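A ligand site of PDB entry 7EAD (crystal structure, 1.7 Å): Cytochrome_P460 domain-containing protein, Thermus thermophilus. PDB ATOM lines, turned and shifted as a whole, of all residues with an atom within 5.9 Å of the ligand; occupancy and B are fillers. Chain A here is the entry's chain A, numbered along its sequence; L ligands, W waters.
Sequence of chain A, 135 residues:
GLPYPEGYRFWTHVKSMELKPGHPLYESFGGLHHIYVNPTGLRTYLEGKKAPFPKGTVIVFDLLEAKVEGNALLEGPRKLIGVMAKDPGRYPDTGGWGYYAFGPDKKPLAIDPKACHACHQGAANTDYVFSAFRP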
ATOM      1  N   LYS A  15      17.803  19.231  20.750  1.00  0.00           N
ATOM      2  CA  LYS A  15      17.232  19.891  19.578  1.00  0.00           C
ATOM      3  C   LYS A  15      18.360  20.167  18.601  1.00  0.00           C
ATOM      4  O   LYS A  15      19.543  20.007  18.913  1.00  0.00           O
ATOM      5  CB  LYS A  15      16.526  21.190  19.954  1.00  0.00           C
ATOM      6  CG  LYS A  15      17.492  22.254  20.443  1.00  0.00           C
ATOM      7  CD  LYS A  15      16.793  23.589  20.704  1.00  0.00           C
ATOM      8  CE  LYS A  15      16.303  24.206  19.392  1.00  0.00           C
ATOM      9  NZ  LYS A  15      15.630  25.515  19.692  1.00  0.00           N
ATOM     10  N   SER A  16      17.969  20.600  17.396  1.00  0.00           N
ATOM     11  CA  SER A  16      18.903  21.055  16.378  1.00  0.00           C
ATOM     12  C   SER A  16      18.353  22.349  15.785  1.00  0.00           C
ATOM     13  O   SER A  16      17.165  22.636  15.890  1.00  0.00           O
ATOM     14  CB  SER A  16      19.107  20.012  15.283  1.00  0.00           C
ATOM     15  OG  SER A  16      19.527  18.776  15.855  1.00  0.00           O
ATOM     16  N   MET A  17      19.236  23.068  15.134  1.00  0.00           N
ATOM     17  CA  MET A  17      18.870  24.306  14.503  1.00  0.00           C
ATOM     18  C   MET A  17      19.981  24.813  13.600  1.00  0.00           C
ATOM     19  O   MET A  17      21.080  24.690  13.932  1.00  0.00           O
ATOM     20  CB  MET A  17      18.582  25.359  15.568  1.00  0.00           C
ATOM     21  CG  MET A  17      17.948  26.635  15.092  1.00  0.00           C
ATOM     22  SD  MET A  17      17.795  27.861  16.418  1.00  0.00           S
ATOM     23  CE  MET A  17      16.730  29.020  15.663  1.00  0.00           C
ATOM     24  N   LEU A  25      23.237  35.867  15.006  1.00  0.00           N
ATOM     25  CA  LEU A  25      24.237  34.974  15.587  1.00  0.00           C
ATOM     26  C   LEU A  25      25.040  34.233  14.529  1.00  0.00           C
ATOM     27  O   LEU A  25      25.791  33.308  14.866  1.00  0.00           O
ATOM     28  CB  LEU A  25      23.572  33.977  16.545  1.00  0.00           C
ATOM     29  CG  LEU A  25      22.837  34.554  17.770  1.00  0.00           C
ATOM     30  CD1 LEU A  25      22.302  33.439  18.661  1.00  0.00           C
ATOM     31  CD2 LEU A  25      23.752  35.447  18.545  1.00  0.00           C
ATOM     32  N   PHE A  29      27.951  31.830  15.690  1.00  0.00           N
ATOM     33  CA  PHE A  29      27.494  30.443  15.747  1.00  0.00           C
ATOM     34  C   PHE A  29      26.838  29.984  14.446  1.00  0.00           C
ATOM     35  O   PHE A  29      25.985  29.090  14.479  1.00  0.00           O
ATOM     36  CB  PHE A  29      26.515  30.233  16.907  1.00  0.00           C
ATOM     37  CG  PHE A  29      27.065  30.621  18.233  1.00  0.00           C
ATOM     38  CD1 PHE A  29      27.946  29.801  18.907  1.00  0.00           C
ATOM     39  CD2 PHE A  29      26.678  31.817  18.833  1.00  0.00           C
ATOM     40  CE1 PHE A  29      28.451  30.146  20.140  1.00  0.00           C
ATOM     41  CE2 PHE A  29      27.179  32.175  20.066  1.00  0.00           C
ATOM     42  CZ  PHE A  29      28.067  31.333  20.720  1.00  0.00           C
ATOM     43  N   HIS A  33      23.749  23.401  14.338  1.00  0.00           N
ATOM     44  CA  HIS A  33      24.158  22.992  15.664  1.00  0.00           C
ATOM     45  C   HIS A  33      23.152  22.016  16.282  1.00  0.00           C
ATOM     46  O   HIS A  33      21.955  22.035  16.001  1.00  0.00           O
ATOM     47  CB  HIS A  33      24.392  24.213  16.592  1.00  0.00           C
ATOM     48  CG  HIS A  33      23.150  24.923  17.038  1.00  0.00           C
ATOM     49  ND1 HIS A  33      22.722  26.113  16.469  1.00  0.00           N
ATOM     50  CD2 HIS A  33      22.259  24.654  18.031  1.00  0.00           C
ATOM     51  CE1 HIS A  33      21.628  26.526  17.076  1.00  0.00           C
ATOM     52  NE2 HIS A  33      21.324  25.656  18.022  1.00  0.00           N
ATOM     53  N   ILE A  35      22.238  20.318  20.189  1.00  0.00           N
ATOM     54  CA  ILE A  35      22.406  20.492  21.618  1.00  0.00           C
ATOM     55  C   ILE A  35      22.245  19.126  22.277  1.00  0.00           C
ATOM     56  O   ILE A  35      21.360  18.346  21.901  1.00  0.00           O
ATOM     57  CB  ILE A  35      21.409  21.537  22.163  1.00  0.00           C
ATOM     58  CG1 ILE A  35      21.838  22.918  21.664  1.00  0.00           C
ATOM     59  CG2 ILE A  35      21.364  21.523  23.696  1.00  0.00           C
ATOM     60  CD1 ILE A  35      20.771  24.002  21.746  1.00  0.00           C
ATOM     61  N   TYR A  45      15.108  19.369  31.598  1.00  0.00           N
ATOM     62  CA  TYR A  45      14.595  19.630  30.261  1.00  0.00           C
ATOM     63  C   TYR A  45      13.225  18.991  30.059  1.00  0.00           C
ATOM     64  O   TYR A  45      12.303  19.631  29.546  1.00  0.00           O
ATOM     65  CB  TYR A  45      15.581  19.089  29.229  1.00  0.00           C
ATOM     66  CG  TYR A  45      16.613  20.040  28.650  1.00  0.00           C
ATOM     67  CD1 TYR A  45      16.238  21.146  27.900  1.00  0.00           C
ATOM     68  CD2 TYR A  45      17.967  19.779  28.811  1.00  0.00           C
ATOM     69  CE1 TYR A  45      17.194  21.997  27.344  1.00  0.00           C
ATOM     70  CE2 TYR A  45      18.927  20.610  28.265  1.00  0.00           C
ATOM     71  CZ  TYR A  45      18.543  21.714  27.514  1.00  0.00           C
ATOM     72  OH  TYR A  45      19.511  22.518  26.970  1.00  0.00           O
ATOM     73  N   ILE A  59      25.660  20.779  29.456  1.00  0.00           N
ATOM     74  CA  ILE A  59      24.988  20.929  28.173  1.00  0.00           C
ATOM     75  C   ILE A  59      26.020  21.335  27.137  1.00  0.00           C
ATOM     76  O   ILE A  59      26.897  22.162  27.409  1.00  0.00           O
ATOM     77  CB  ILE A  59      23.844  21.954  28.247  1.00  0.00           C
ATOM     78  CG1 ILE A  59      22.923  21.644  29.432  1.00  0.00           C
ATOM     79  CG2 ILE A  59      23.057  21.966  26.937  1.00  0.00           C
ATOM     80  CD1 ILE A  59      21.990  22.797  29.768  1.00  0.00           C
ATOM     81  N   VAL A  60      25.936  20.743  25.953  1.00  0.00           N
ATOM     82  CA  VAL A  60      26.906  20.968  24.897  1.00  0.00           C
ATOM     83  C   VAL A  60      26.193  21.478  23.655  1.00  0.00           C
ATOM     84  O   VAL A  60      25.216  20.893  23.194  1.00  0.00           O
ATOM     85  CB  VAL A  60      27.734  19.706  24.569  1.00  0.00           C
ATOM     86  CG1 VAL A  60      28.683  20.020  23.421  1.00  0.00           C
ATOM     87  CG2 VAL A  60      28.498  19.233  25.820  1.00  0.00           C
ATOM     88  N   PHE A  61      26.686  22.597  23.152  1.00  0.00           N
ATOM     89  CA  PHE A  61      26.238  23.202  21.901  1.00  0.00           C
ATOM     90  C   PHE A  61      27.255  22.777  20.841  1.00  0.00           C
ATOM     91  O   PHE A  61      28.400  23.254  20.846  1.00  0.00           O
ATOM     92  CB  PHE A  61      26.180  24.708  22.110  1.00  0.00           C
ATOM     93  CG  PHE A  61      25.749  25.506  20.910  1.00  0.00           C
ATOM     94  CD1 PHE A  61      26.620  25.710  19.842  1.00  0.00           C
ATOM     95  CD2 PHE A  61      24.514  26.129  20.893  1.00  0.00           C
ATOM     96  CE1 PHE A  61      26.243  26.482  18.754  1.00  0.00           C
ATOM     97  CE2 PHE A  61      24.125  26.905  19.797  1.00  0.00           C
ATOM     98  CZ  PHE A  61      24.996  27.073  18.739  1.00  0.00           C
ATOM     99  N   ILE A  81      32.536  23.467  19.953  1.00  0.00           N
ATOM    100  CA  ILE A  81      31.468  23.168  20.900  1.00  0.00           C
ATOM    101  C   ILE A  81      31.454  24.245  21.963  1.00  0.00           C
ATOM    102  O   ILE A  81      32.502  24.770  22.362  1.00  0.00           O
ATOM    103  CB  ILE A  81      31.597  21.770  21.547  1.00  0.00           C
ATOM    104  CG1 ILE A  81      32.798  21.684  22.502  1.00  0.00           C
ATOM    105  CG2 ILE A  81      31.656  20.683  20.482  1.00  0.00           C
ATOM    106  CD1 ILE A  81      32.854  20.374  23.287  1.00  0.00           C
ATOM    107  N   GLY A  82      30.246  24.616  22.387  1.00  0.00           N
ATOM    108  CA  GLY A  82      30.056  25.407  23.586  1.00  0.00           C
ATOM    109  C   GLY A  82      29.556  24.466  24.665  1.00  0.00           C
ATOM    110  O   GLY A  82      28.905  23.465  24.380  1.00  0.00           O
ATOM    111  N   VAL A  83      29.900  24.790  25.910  1.00  0.00           N
ATOM    112  CA  VAL A  83      29.603  23.926  27.055  1.00  0.00           C
ATOM    113  C   VAL A  83      29.099  24.809  28.189  1.00  0.00           C
ATOM    114  O   VAL A  83      29.673  25.868  28.443  1.00  0.00           O
ATOM    115  CB  VAL A  83      30.842  23.132  27.504  1.00  0.00           C
ATOM    116  CG1 VAL A  83      30.479  22.143  28.611  1.00  0.00           C
ATOM    117  CG2 VAL A  83      31.494  22.402  26.313  1.00  0.00           C
ATOM    118  N   MET A  84      28.019  24.389  28.831  1.00  0.00           N
ATOM    119  CA  MET A  84      27.559  24.984  30.075  1.00  0.00           C
ATOM    120  C   MET A  84      27.529  23.891  31.129  1.00  0.00           C
ATOM    121  O   MET A  84      26.921  22.835  30.923  1.00  0.00           O
ATOM    122  CB  MET A  84      26.177  25.605  29.913  1.00  0.00           C
ATOM    123  CG  MET A  84      26.199  26.930  29.140  1.00  0.00           C
ATOM    124  SD  MET A  84      24.546  27.425  28.676  1.00  0.00           S
ATOM    125  CE  MET A  84      23.861  27.903  30.268  1.00  0.00           C
ATOM    126  N   TYR A  99      30.775  28.529  31.708  1.00  0.00           N
ATOM    127  CA  TYR A  99      30.754  28.613  30.257  1.00  0.00           C
ATOM    128  C   TYR A  99      32.140  28.295  29.714  1.00  0.00           C
ATOM    129  O   TYR A  99      33.132  28.910  30.132  1.00  0.00           O
ATOM    130  CB  TYR A  99      30.328  29.999  29.795  1.00  0.00           C
ATOM    131  CG  TYR A  99      28.907  30.363  30.147  1.00  0.00           C
ATOM    132  CD1 TYR A  99      28.613  31.001  31.357  1.00  0.00           C
ATOM    133  CD2 TYR A  99      27.862  30.102  29.272  1.00  0.00           C
ATOM    134  CE1 TYR A  99      27.317  31.338  31.678  1.00  0.00           C
ATOM    135  CE2 TYR A  99      26.565  30.439  29.593  1.00  0.00           C
ATOM    136  CZ  TYR A  99      26.295  31.068  30.791  1.00  0.00           C
ATOM    137  OH  TYR A  99      24.999  31.405  31.112  1.00  0.00           O
ATOM    138  N   TYR A 100      32.204  27.353  28.766  1.00  0.00           N
ATOM    139  CA  TYR A 100      33.455  26.892  28.195  1.00  0.00           C
ATOM    140  C   TYR A 100      33.257  26.651  26.706  1.00  0.00           C
ATOM    141  O   TYR A 100      32.129  26.458  26.240  1.00  0.00           O
ATOM    142  CB  TYR A 100      33.940  25.588  28.883  1.00  0.00           C
ATOM    143  CG  TYR A 100      34.260  25.771  30.343  1.00  0.00           C
ATOM    144  CD1 TYR A 100      35.518  26.215  30.744  1.00  0.00           C
ATOM    145  CD2 TYR A 100      33.311  25.523  31.324  1.00  0.00           C
ATOM    146  CE1 TYR A 100      35.826  26.390  32.082  1.00  0.00           C
ATOM    147  CE2 TYR A 100      33.608  25.696  32.676  1.00  0.00           C
ATOM    148  CZ  TYR A 100      34.871  26.130  33.042  1.00  0.00           C
ATOM    149  OH  TYR A 100      35.177  26.312  34.373  1.00  0.00           O
ATOM    150  N   ALA A 101      34.361  26.634  25.963  1.00  0.00           N
ATOM    151  CA  ALA A 101      34.296  26.312  24.554  1.00  0.00           C
ATOM    152  C   ALA A 101      35.544  25.529  24.163  1.00  0.00           C
ATOM    153  O   ALA A 101      36.614  25.723  24.732  1.00  0.00           O
ATOM    154  CB  ALA A 101      34.160  27.586  23.701  1.00  0.00           C
ATOM    155  N   ILE A 111      37.633  32.294  25.522  1.00  0.00           N
ATOM    156  CA  ILE A 111      36.339  32.950  25.477  1.00  0.00           C
ATOM    157  C   ILE A 111      36.250  33.948  26.619  1.00  0.00           C
ATOM    158  O   ILE A 111      37.091  33.970  27.517  1.00  0.00           O
ATOM    159  CB  ILE A 111      35.162  31.941  25.552  1.00  0.00           C
ATOM    160  CG1 ILE A 111      35.196  31.201  26.883  1.00  0.00           C
ATOM    161  CG2 ILE A 111      35.201  30.984  24.361  1.00  0.00           C
ATOM    162  CD1 ILE A 111      33.908  30.466  27.214  1.00  0.00           C
ATOM    163  N   ASP A 112      35.212  34.768  26.559  1.00  0.00           N
ATOM    164  CA  ASP A 112      34.843  35.614  27.691  1.00  0.00           C
ATOM    165  C   ASP A 112      33.576  35.051  28.302  1.00  0.00           C
ATOM    166  O   ASP A 112      32.467  35.349  27.829  1.00  0.00           O
ATOM    167  CB  ASP A 112      34.631  37.052  27.234  1.00  0.00           C
ATOM    168  CG  ASP A 112      34.292  37.974  28.384  1.00  0.00           C
ATOM    169  OD1 ASP A 112      34.231  37.493  29.539  1.00  0.00           O
ATOM    170  OD2 ASP A 112      34.091  39.183  28.129  1.00  0.00           O
ATOM    171  N   PRO A 113      33.660  34.256  29.371  1.00  0.00           N
ATOM    172  CA  PRO A 113      32.425  33.659  29.922  1.00  0.00           C
ATOM    173  C   PRO A 113      31.416  34.691  30.368  1.00  0.00           C
ATOM    174  O   PRO A 113      30.208  34.417  30.293  1.00  0.00           O
ATOM    175  CB  PRO A 113      32.941  32.824  31.104  1.00  0.00           C
ATOM    176  CG  PRO A 113      34.217  33.469  31.483  1.00  0.00           C
ATOM    177  CD  PRO A 113      34.834  33.920  30.193  1.00  0.00           C
ATOM    178  N   ALA A 115      30.674  37.308  28.752  1.00  0.00           N
ATOM    179  CA  ALA A 115      29.942  37.661  27.541  1.00  0.00           C
ATOM    180  C   ALA A 115      28.971  36.560  27.141  1.00  0.00           C
ATOM    181  O   ALA A 115      27.864  36.851  26.661  1.00  0.00           O
ATOM    182  CB  ALA A 115      30.929  37.950  26.405  1.00  0.00           C
ATOM    183  N   CYS A 116      29.339  35.287  27.327  1.00  0.00           N
ATOM    184  CA  CYS A 116      28.382  34.211  27.139  1.00  0.00           C
ATOM    185  C   CYS A 116      27.176  34.414  28.038  1.00  0.00           C
ATOM    186  O   CYS A 116      26.026  34.371  27.580  1.00  0.00           O
ATOM    187  CB  CYS A 116      29.015  32.854  27.458  1.00  0.00           C
ATOM    188  SG  CYS A 116      30.607  32.438  26.682  1.00  0.00           S
ATOM    189  N   HIS A 117      27.424  34.621  29.335  1.00  0.00           N
ATOM    190  CA  HIS A 117      26.343  34.739  30.299  1.00  0.00           C
ATOM    191  C   HIS A 117      25.499  35.978  30.052  1.00  0.00           C
ATOM    192  O   HIS A 117      24.281  35.948  30.242  1.00  0.00           O
ATOM    193  CB  HIS A 117      26.946  34.736  31.701  1.00  0.00           C
ATOM    194  CG  HIS A 117      25.929  34.715  32.787  1.00  0.00           C
ATOM    195  ND1 HIS A 117      25.070  33.658  32.989  1.00  0.00           N
ATOM    196  CD2 HIS A 117      25.608  35.644  33.732  1.00  0.00           C
ATOM    197  CE1 HIS A 117      24.277  33.921  34.020  1.00  0.00           C
ATOM    198  NE2 HIS A 117      24.582  35.124  34.478  1.00  0.00           N
ATOM    199  N   CYS A 119      24.442  37.295  27.287  1.00  0.00           N
ATOM    200  CA  CYS A 119      23.342  36.972  26.385  1.00  0.00           C
ATOM    201  C   CYS A 119      22.411  35.950  27.005  1.00  0.00           C
ATOM    202  O   CYS A 119      21.179  36.037  26.837  1.00  0.00           O
ATOM    203  CB  CYS A 119      23.905  36.434  25.066  1.00  0.00           C
ATOM    204  SG  CYS A 119      22.640  36.052  23.857  1.00  0.00           S
ATOM    205  N   HIS A 120      22.957  34.946  27.718  1.00  0.00           N
ATOM    206  CA  HIS A 120      22.124  33.911  28.310  1.00  0.00           C
ATOM    207  C   HIS A 120      21.270  34.447  29.445  1.00  0.00           C
ATOM    208  O   HIS A 120      20.283  33.820  29.810  1.00  0.00           O
ATOM    209  CB  HIS A 120      22.981  32.728  28.796  1.00  0.00           C
ATOM    210  CG  HIS A 120      23.322  31.753  27.707  1.00  0.00           C
ATOM    211  ND1 HIS A 120      22.695  30.523  27.583  1.00  0.00           N
ATOM    212  CD2 HIS A 120      24.205  31.833  26.692  1.00  0.00           C
ATOM    213  CE1 HIS A 120      23.186  29.895  26.528  1.00  0.00           C
ATOM    214  NE2 HIS A 120      24.102  30.661  25.976  1.00  0.00           N
ATOM    215  N   TYR A 128      18.834  30.201  32.571  1.00  0.00           N
ATOM    216  CA  TYR A 128      19.851  30.679  31.636  1.00  0.00           C
ATOM    217  C   TYR A 128      20.057  29.754  30.455  1.00  0.00           C
ATOM    218  O   TYR A 128      21.060  29.868  29.759  1.00  0.00           O
ATOM    219  CB  TYR A 128      21.185  30.907  32.342  1.00  0.00           C
ATOM    220  CG  TYR A 128      21.047  31.855  33.491  1.00  0.00           C
ATOM    221  CD1 TYR A 128      20.892  33.227  33.270  1.00  0.00           C
ATOM    222  CD2 TYR A 128      21.016  31.389  34.796  1.00  0.00           C
ATOM    223  CE1 TYR A 128      20.746  34.106  34.338  1.00  0.00           C
ATOM    224  CE2 TYR A 128      20.876  32.247  35.859  1.00  0.00           C
ATOM    225  CZ  TYR A 128      20.737  33.601  35.633  1.00  0.00           C
ATOM    226  OH  TYR A 128      20.599  34.448  36.726  1.00  0.00           O
ATOM    227  N   VAL A 129      19.089  28.875  30.208  1.00  0.00           N
ATOM    228  CA  VAL A 129      19.134  27.920  29.096  1.00  0.00           C
ATOM    229  C   VAL A 129      18.017  28.264  28.128  1.00  0.00           C
ATOM    230  O   VAL A 129      16.845  28.295  28.516  1.00  0.00           O
ATOM    231  CB  VAL A 129      19.013  26.477  29.608  1.00  0.00           C
ATOM    232  CG1 VAL A 129      18.857  25.510  28.418  1.00  0.00           C
ATOM    233  CG2 VAL A 129      20.212  26.121  30.448  1.00  0.00           C
ATOM    234  N   PHE A 130      18.378  28.509  26.871  1.00  0.00           N
ATOM    235  CA  PHE A 130      17.412  28.882  25.847  1.00  0.00           C
ATOM    236  C   PHE A 130      16.664  27.681  25.300  1.00  0.00           C
ATOM    237  O   PHE A 130      15.430  27.686  25.209  1.00  0.00           O
ATOM    238  CB  PHE A 130      18.107  29.588  24.686  1.00  0.00           C
ATOM    239  CG  PHE A 130      18.609  30.965  25.004  1.00  0.00           C
ATOM    240  CD1 PHE A 130      17.735  32.033  25.066  1.00  0.00           C
ATOM    241  CD2 PHE A 130      19.950  31.195  25.177  1.00  0.00           C
ATOM    242  CE1 PHE A 130      18.206  33.308  25.331  1.00  0.00           C
ATOM    243  CE2 PHE A 130      20.439  32.444  25.432  1.00  0.00           C
ATOM    244  CZ  PHE A 130      19.553  33.518  25.500  1.00  0.00           C
ATOM    245  N   SER A 131      17.408  26.666  24.862  1.00  0.00           N
ATOM    246  CA  SER A 131      16.846  25.538  24.159  1.00  0.00           C
ATOM    247  C   SER A 131      15.806  24.825  25.011  1.00  0.00           C
ATOM    248  O   SER A 131      15.893  24.767  26.237  1.00  0.00           O
ATOM    249  CB  SER A 131      17.926  24.539  23.766  1.00  0.00           C
ATOM    250  OG  SER A 131      18.723  24.195  24.895  1.00  0.00           O
ATOM    251  N   ALA A 132      14.789  24.311  24.328  1.00  0.00           N
ATOM    252  CA  ALA A 132      13.777  23.439  24.902  1.00  0.00           C
ATOM    253  C   ALA A 132      13.938  22.049  24.301  1.00  0.00           C
ATOM    254  O   ALA A 132      14.275  21.918  23.119  1.00  0.00           O
ATOM    255  CB  ALA A 132      12.371  23.977  24.638  1.00  0.00           C
HETATM  256 FE1  LIG L   1      24.859  30.344  23.944  1.00  0.00          FE
HETATM  257  C1  LIG L   1      22.525  27.867  23.390  1.00  0.00           C
HETATM  258  C2  LIG L   1      27.035  27.952  25.164  1.00  0.00           C
HETATM  259  C3  LIG L   1      27.312  32.687  24.132  1.00  0.00           C
HETATM  260  C4  LIG L   1      22.797  32.639  22.440  1.00  0.00           C
HETATM  261  N1  LIG L   1      24.832  28.287  24.146  1.00  0.00           N
HETATM  262  C5  LIG L   1      23.688  27.528  24.041  1.00  0.00           C
HETATM  263  C6  LIG L   1      23.903  26.266  24.706  1.00  0.00           C
HETATM  264  C7  LIG L   1      25.146  26.264  25.203  1.00  0.00           C
HETATM  265  C8  LIG L   1      25.752  27.540  24.860  1.00  0.00           C
HETATM  266  C9  LIG L   1      25.802  25.108  26.006  1.00  0.00           C
HETATM  267  C10 LIG L   1      22.822  25.168  24.809  1.00  0.00           C
HETATM  268  C11 LIG L   1      21.958  25.460  26.046  1.00  0.00           C
HETATM  269  C12 LIG L   1      20.966  26.589  25.839  1.00  0.00           C
HETATM  270  O1  LIG L   1      21.107  27.681  26.457  1.00  0.00           O
HETATM  271  O2  LIG L   1      19.991  26.388  25.079  1.00  0.00           O
HETATM  272  N2  LIG L   1      26.784  30.341  24.526  1.00  0.00           N
HETATM  273  C13 LIG L   1      27.519  29.231  24.976  1.00  0.00           C
HETATM  274  C14 LIG L   1      28.877  29.648  25.207  1.00  0.00           C
HETATM  275  C15 LIG L   1      28.971  30.959  24.931  1.00  0.00           C
HETATM  276  C16 LIG L   1      27.663  31.404  24.496  1.00  0.00           C
HETATM  277  C17 LIG L   1      29.982  28.717  25.763  1.00  0.00           C
HETATM  278  C18 LIG L   1      30.213  31.887  25.052  1.00  0.00           C
HETATM  279  C19 LIG L   1      31.437  31.370  24.284  1.00  0.00           C
HETATM  280  N3  LIG L   1      25.033  32.281  23.356  1.00  0.00           N
HETATM  281  C20 LIG L   1      26.102  33.088  23.644  1.00  0.00           C
HETATM  282  C21 LIG L   1      25.794  34.451  23.220  1.00  0.00           C
HETATM  283  C22 LIG L   1      24.500  34.470  22.825  1.00  0.00           C
HETATM  284  C23 LIG L   1      24.032  33.091  22.852  1.00  0.00           C
HETATM  285  C24 LIG L   1      26.777  35.599  23.540  1.00  0.00           C
HETATM  286  C25 LIG L   1      23.580  35.678  22.397  1.00  0.00           C
HETATM  287  C26 LIG L   1      24.304  36.859  21.722  1.00  0.00           C
HETATM  288  N4  LIG L   1      22.977  30.250  23.052  1.00  0.00           N
HETATM  289  C27 LIG L   1      22.326  31.342  22.482  1.00  0.00           C
HETATM  290  C28 LIG L   1      21.052  30.905  21.959  1.00  0.00           C
HETATM  291  C29 LIG L   1      20.964  29.421  22.249  1.00  0.00           C
HETATM  292  C30 LIG L   1      22.203  29.104  22.918  1.00  0.00           C
HETATM  293  C31 LIG L   1      19.978  31.750  21.248  1.00  0.00           C
HETATM  294  C32 LIG L   1      19.797  28.491  21.892  1.00  0.00           C
HETATM  295  C33 LIG L   1      20.105  27.704  20.623  1.00  0.00           C
HETATM  296  C34 LIG L   1      18.931  26.843  20.232  1.00  0.00           C
HETATM  297  O3  LIG L   1      17.801  27.073  20.736  1.00  0.00           O
HETATM  298  O4  LIG L   1      19.129  25.925  19.384  1.00  0.00           O
HETATM  299  O   HOH W   1      16.520  29.356  21.260  1.00  0.00           O
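N of Ile 35 lies within hydrogen-bond range of O of Lys 15, at 3.0 Å. O of Gly 82 lies within hydrogen-bond range of N of Phe 61. OH of Tyr 45 sits at hydrogen-bond distance from OG of Ser 131 (2.8 Å). O of Met 17 sits at hydrogen-bond distance from N of His 33 (3.0 Å). N of Ile 59 is in hydrogen-bond range of O of Met 84 (2.8 Å). O of Tyr 100 sits at hydrogen-bond distance from N of Val 83, at 2.8 Å. A ring nitrogen (ND1) of His 120 lies within hydrogen-bond range of the backbone carbonyl oxygen of Tyr 128, at 2.8 Å. ND1 of His 120 lies close to SD of Met 84, at 3.8 Å.
SD of Met 17 sits close to O4 of the ligand, at 3.8 Å. CD2 of Leu 25 touches C26 of the ligand, at 3.5 Å. Phe 29 touches the ligand. Ile 35 touches the ligand (CD1 to O4, 3.5 Å). OH of Tyr 45 touches C11 of the ligand (3.9 Å). O of Ile 59 touches C9 of the ligand (3.4 Å). Phe 61 touches the ligand (CD2 to C5, 3.5 Å). Gly 82 touches the ligand (O to C9, 3.9 Å). O of Val 83 touches C17 of the ligand (3.9 Å). Met 84 touches the ligand. Tyr 100 touches the ligand (O to C17, 3.2 Å). Ile 111 touches the ligand. O of Ala 115 touches C24 of the ligand, at 3.5 Å. O of Tyr 128 touches O1 of the ligand (3.96 Å). CA of Val 129 touches O1 of the ligand (3.3 Å). Hydrophobic or aromatic side chains that line the ligand: Met 17, Leu 25, Phe 29, His 33, Ile 35, Ile 59, Phe 61, Met 84, Ile 111, His 120, Val 129 and Phe 130. 22 residues have an atom within 4 Å of the ligand: Lys 15, Met 17, Leu 25, Phe 29, His 33, Ile 35, Tyr 45, Ile 59, Phe 61, Gly 82, Val 83, Met 84, Tyr 100, Ile 111, Ala 115, Cys 116, Cys 119, His 120, Tyr 128, Val 129, Phe 130 and Ser 131. The nearest printed residue that does not touch the ligand is Tyr 99 (4.2 Å).
The side-chain amino group (NZ) of Lys 15 lies within salt-bridge range of an oxygen (O3) of the ligand (2.9 Å). The backbone NH (N) of Phe 130 sits at hydrogen-bond distance from an oxygen (O1) of the ligand. A carbon (C18) of the ligand is bonded to the side-chain sulfur of Cys 116 (1.8 Å). An oxygen (O2) of the ligand lies within hydrogen-bond range of the side-chain hydroxyl (OG) of Ser 131 (2.5 Å). A ring nitrogen (NE2) of His 120 binds an iron atom (FE1) of the ligand (2.2 Å). SG of Cys 119 is bonded to C25 of the ligand (1.8 Å). The backbone NH of Ser 131 is in hydrogen-bond range of an oxygen (O2) of the ligand (2.6 Å). A ring nitrogen (NE2) of His 33 lies within hydrogen-bond range of an oxygen (O4) of the ligand, at 2.6 Å.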
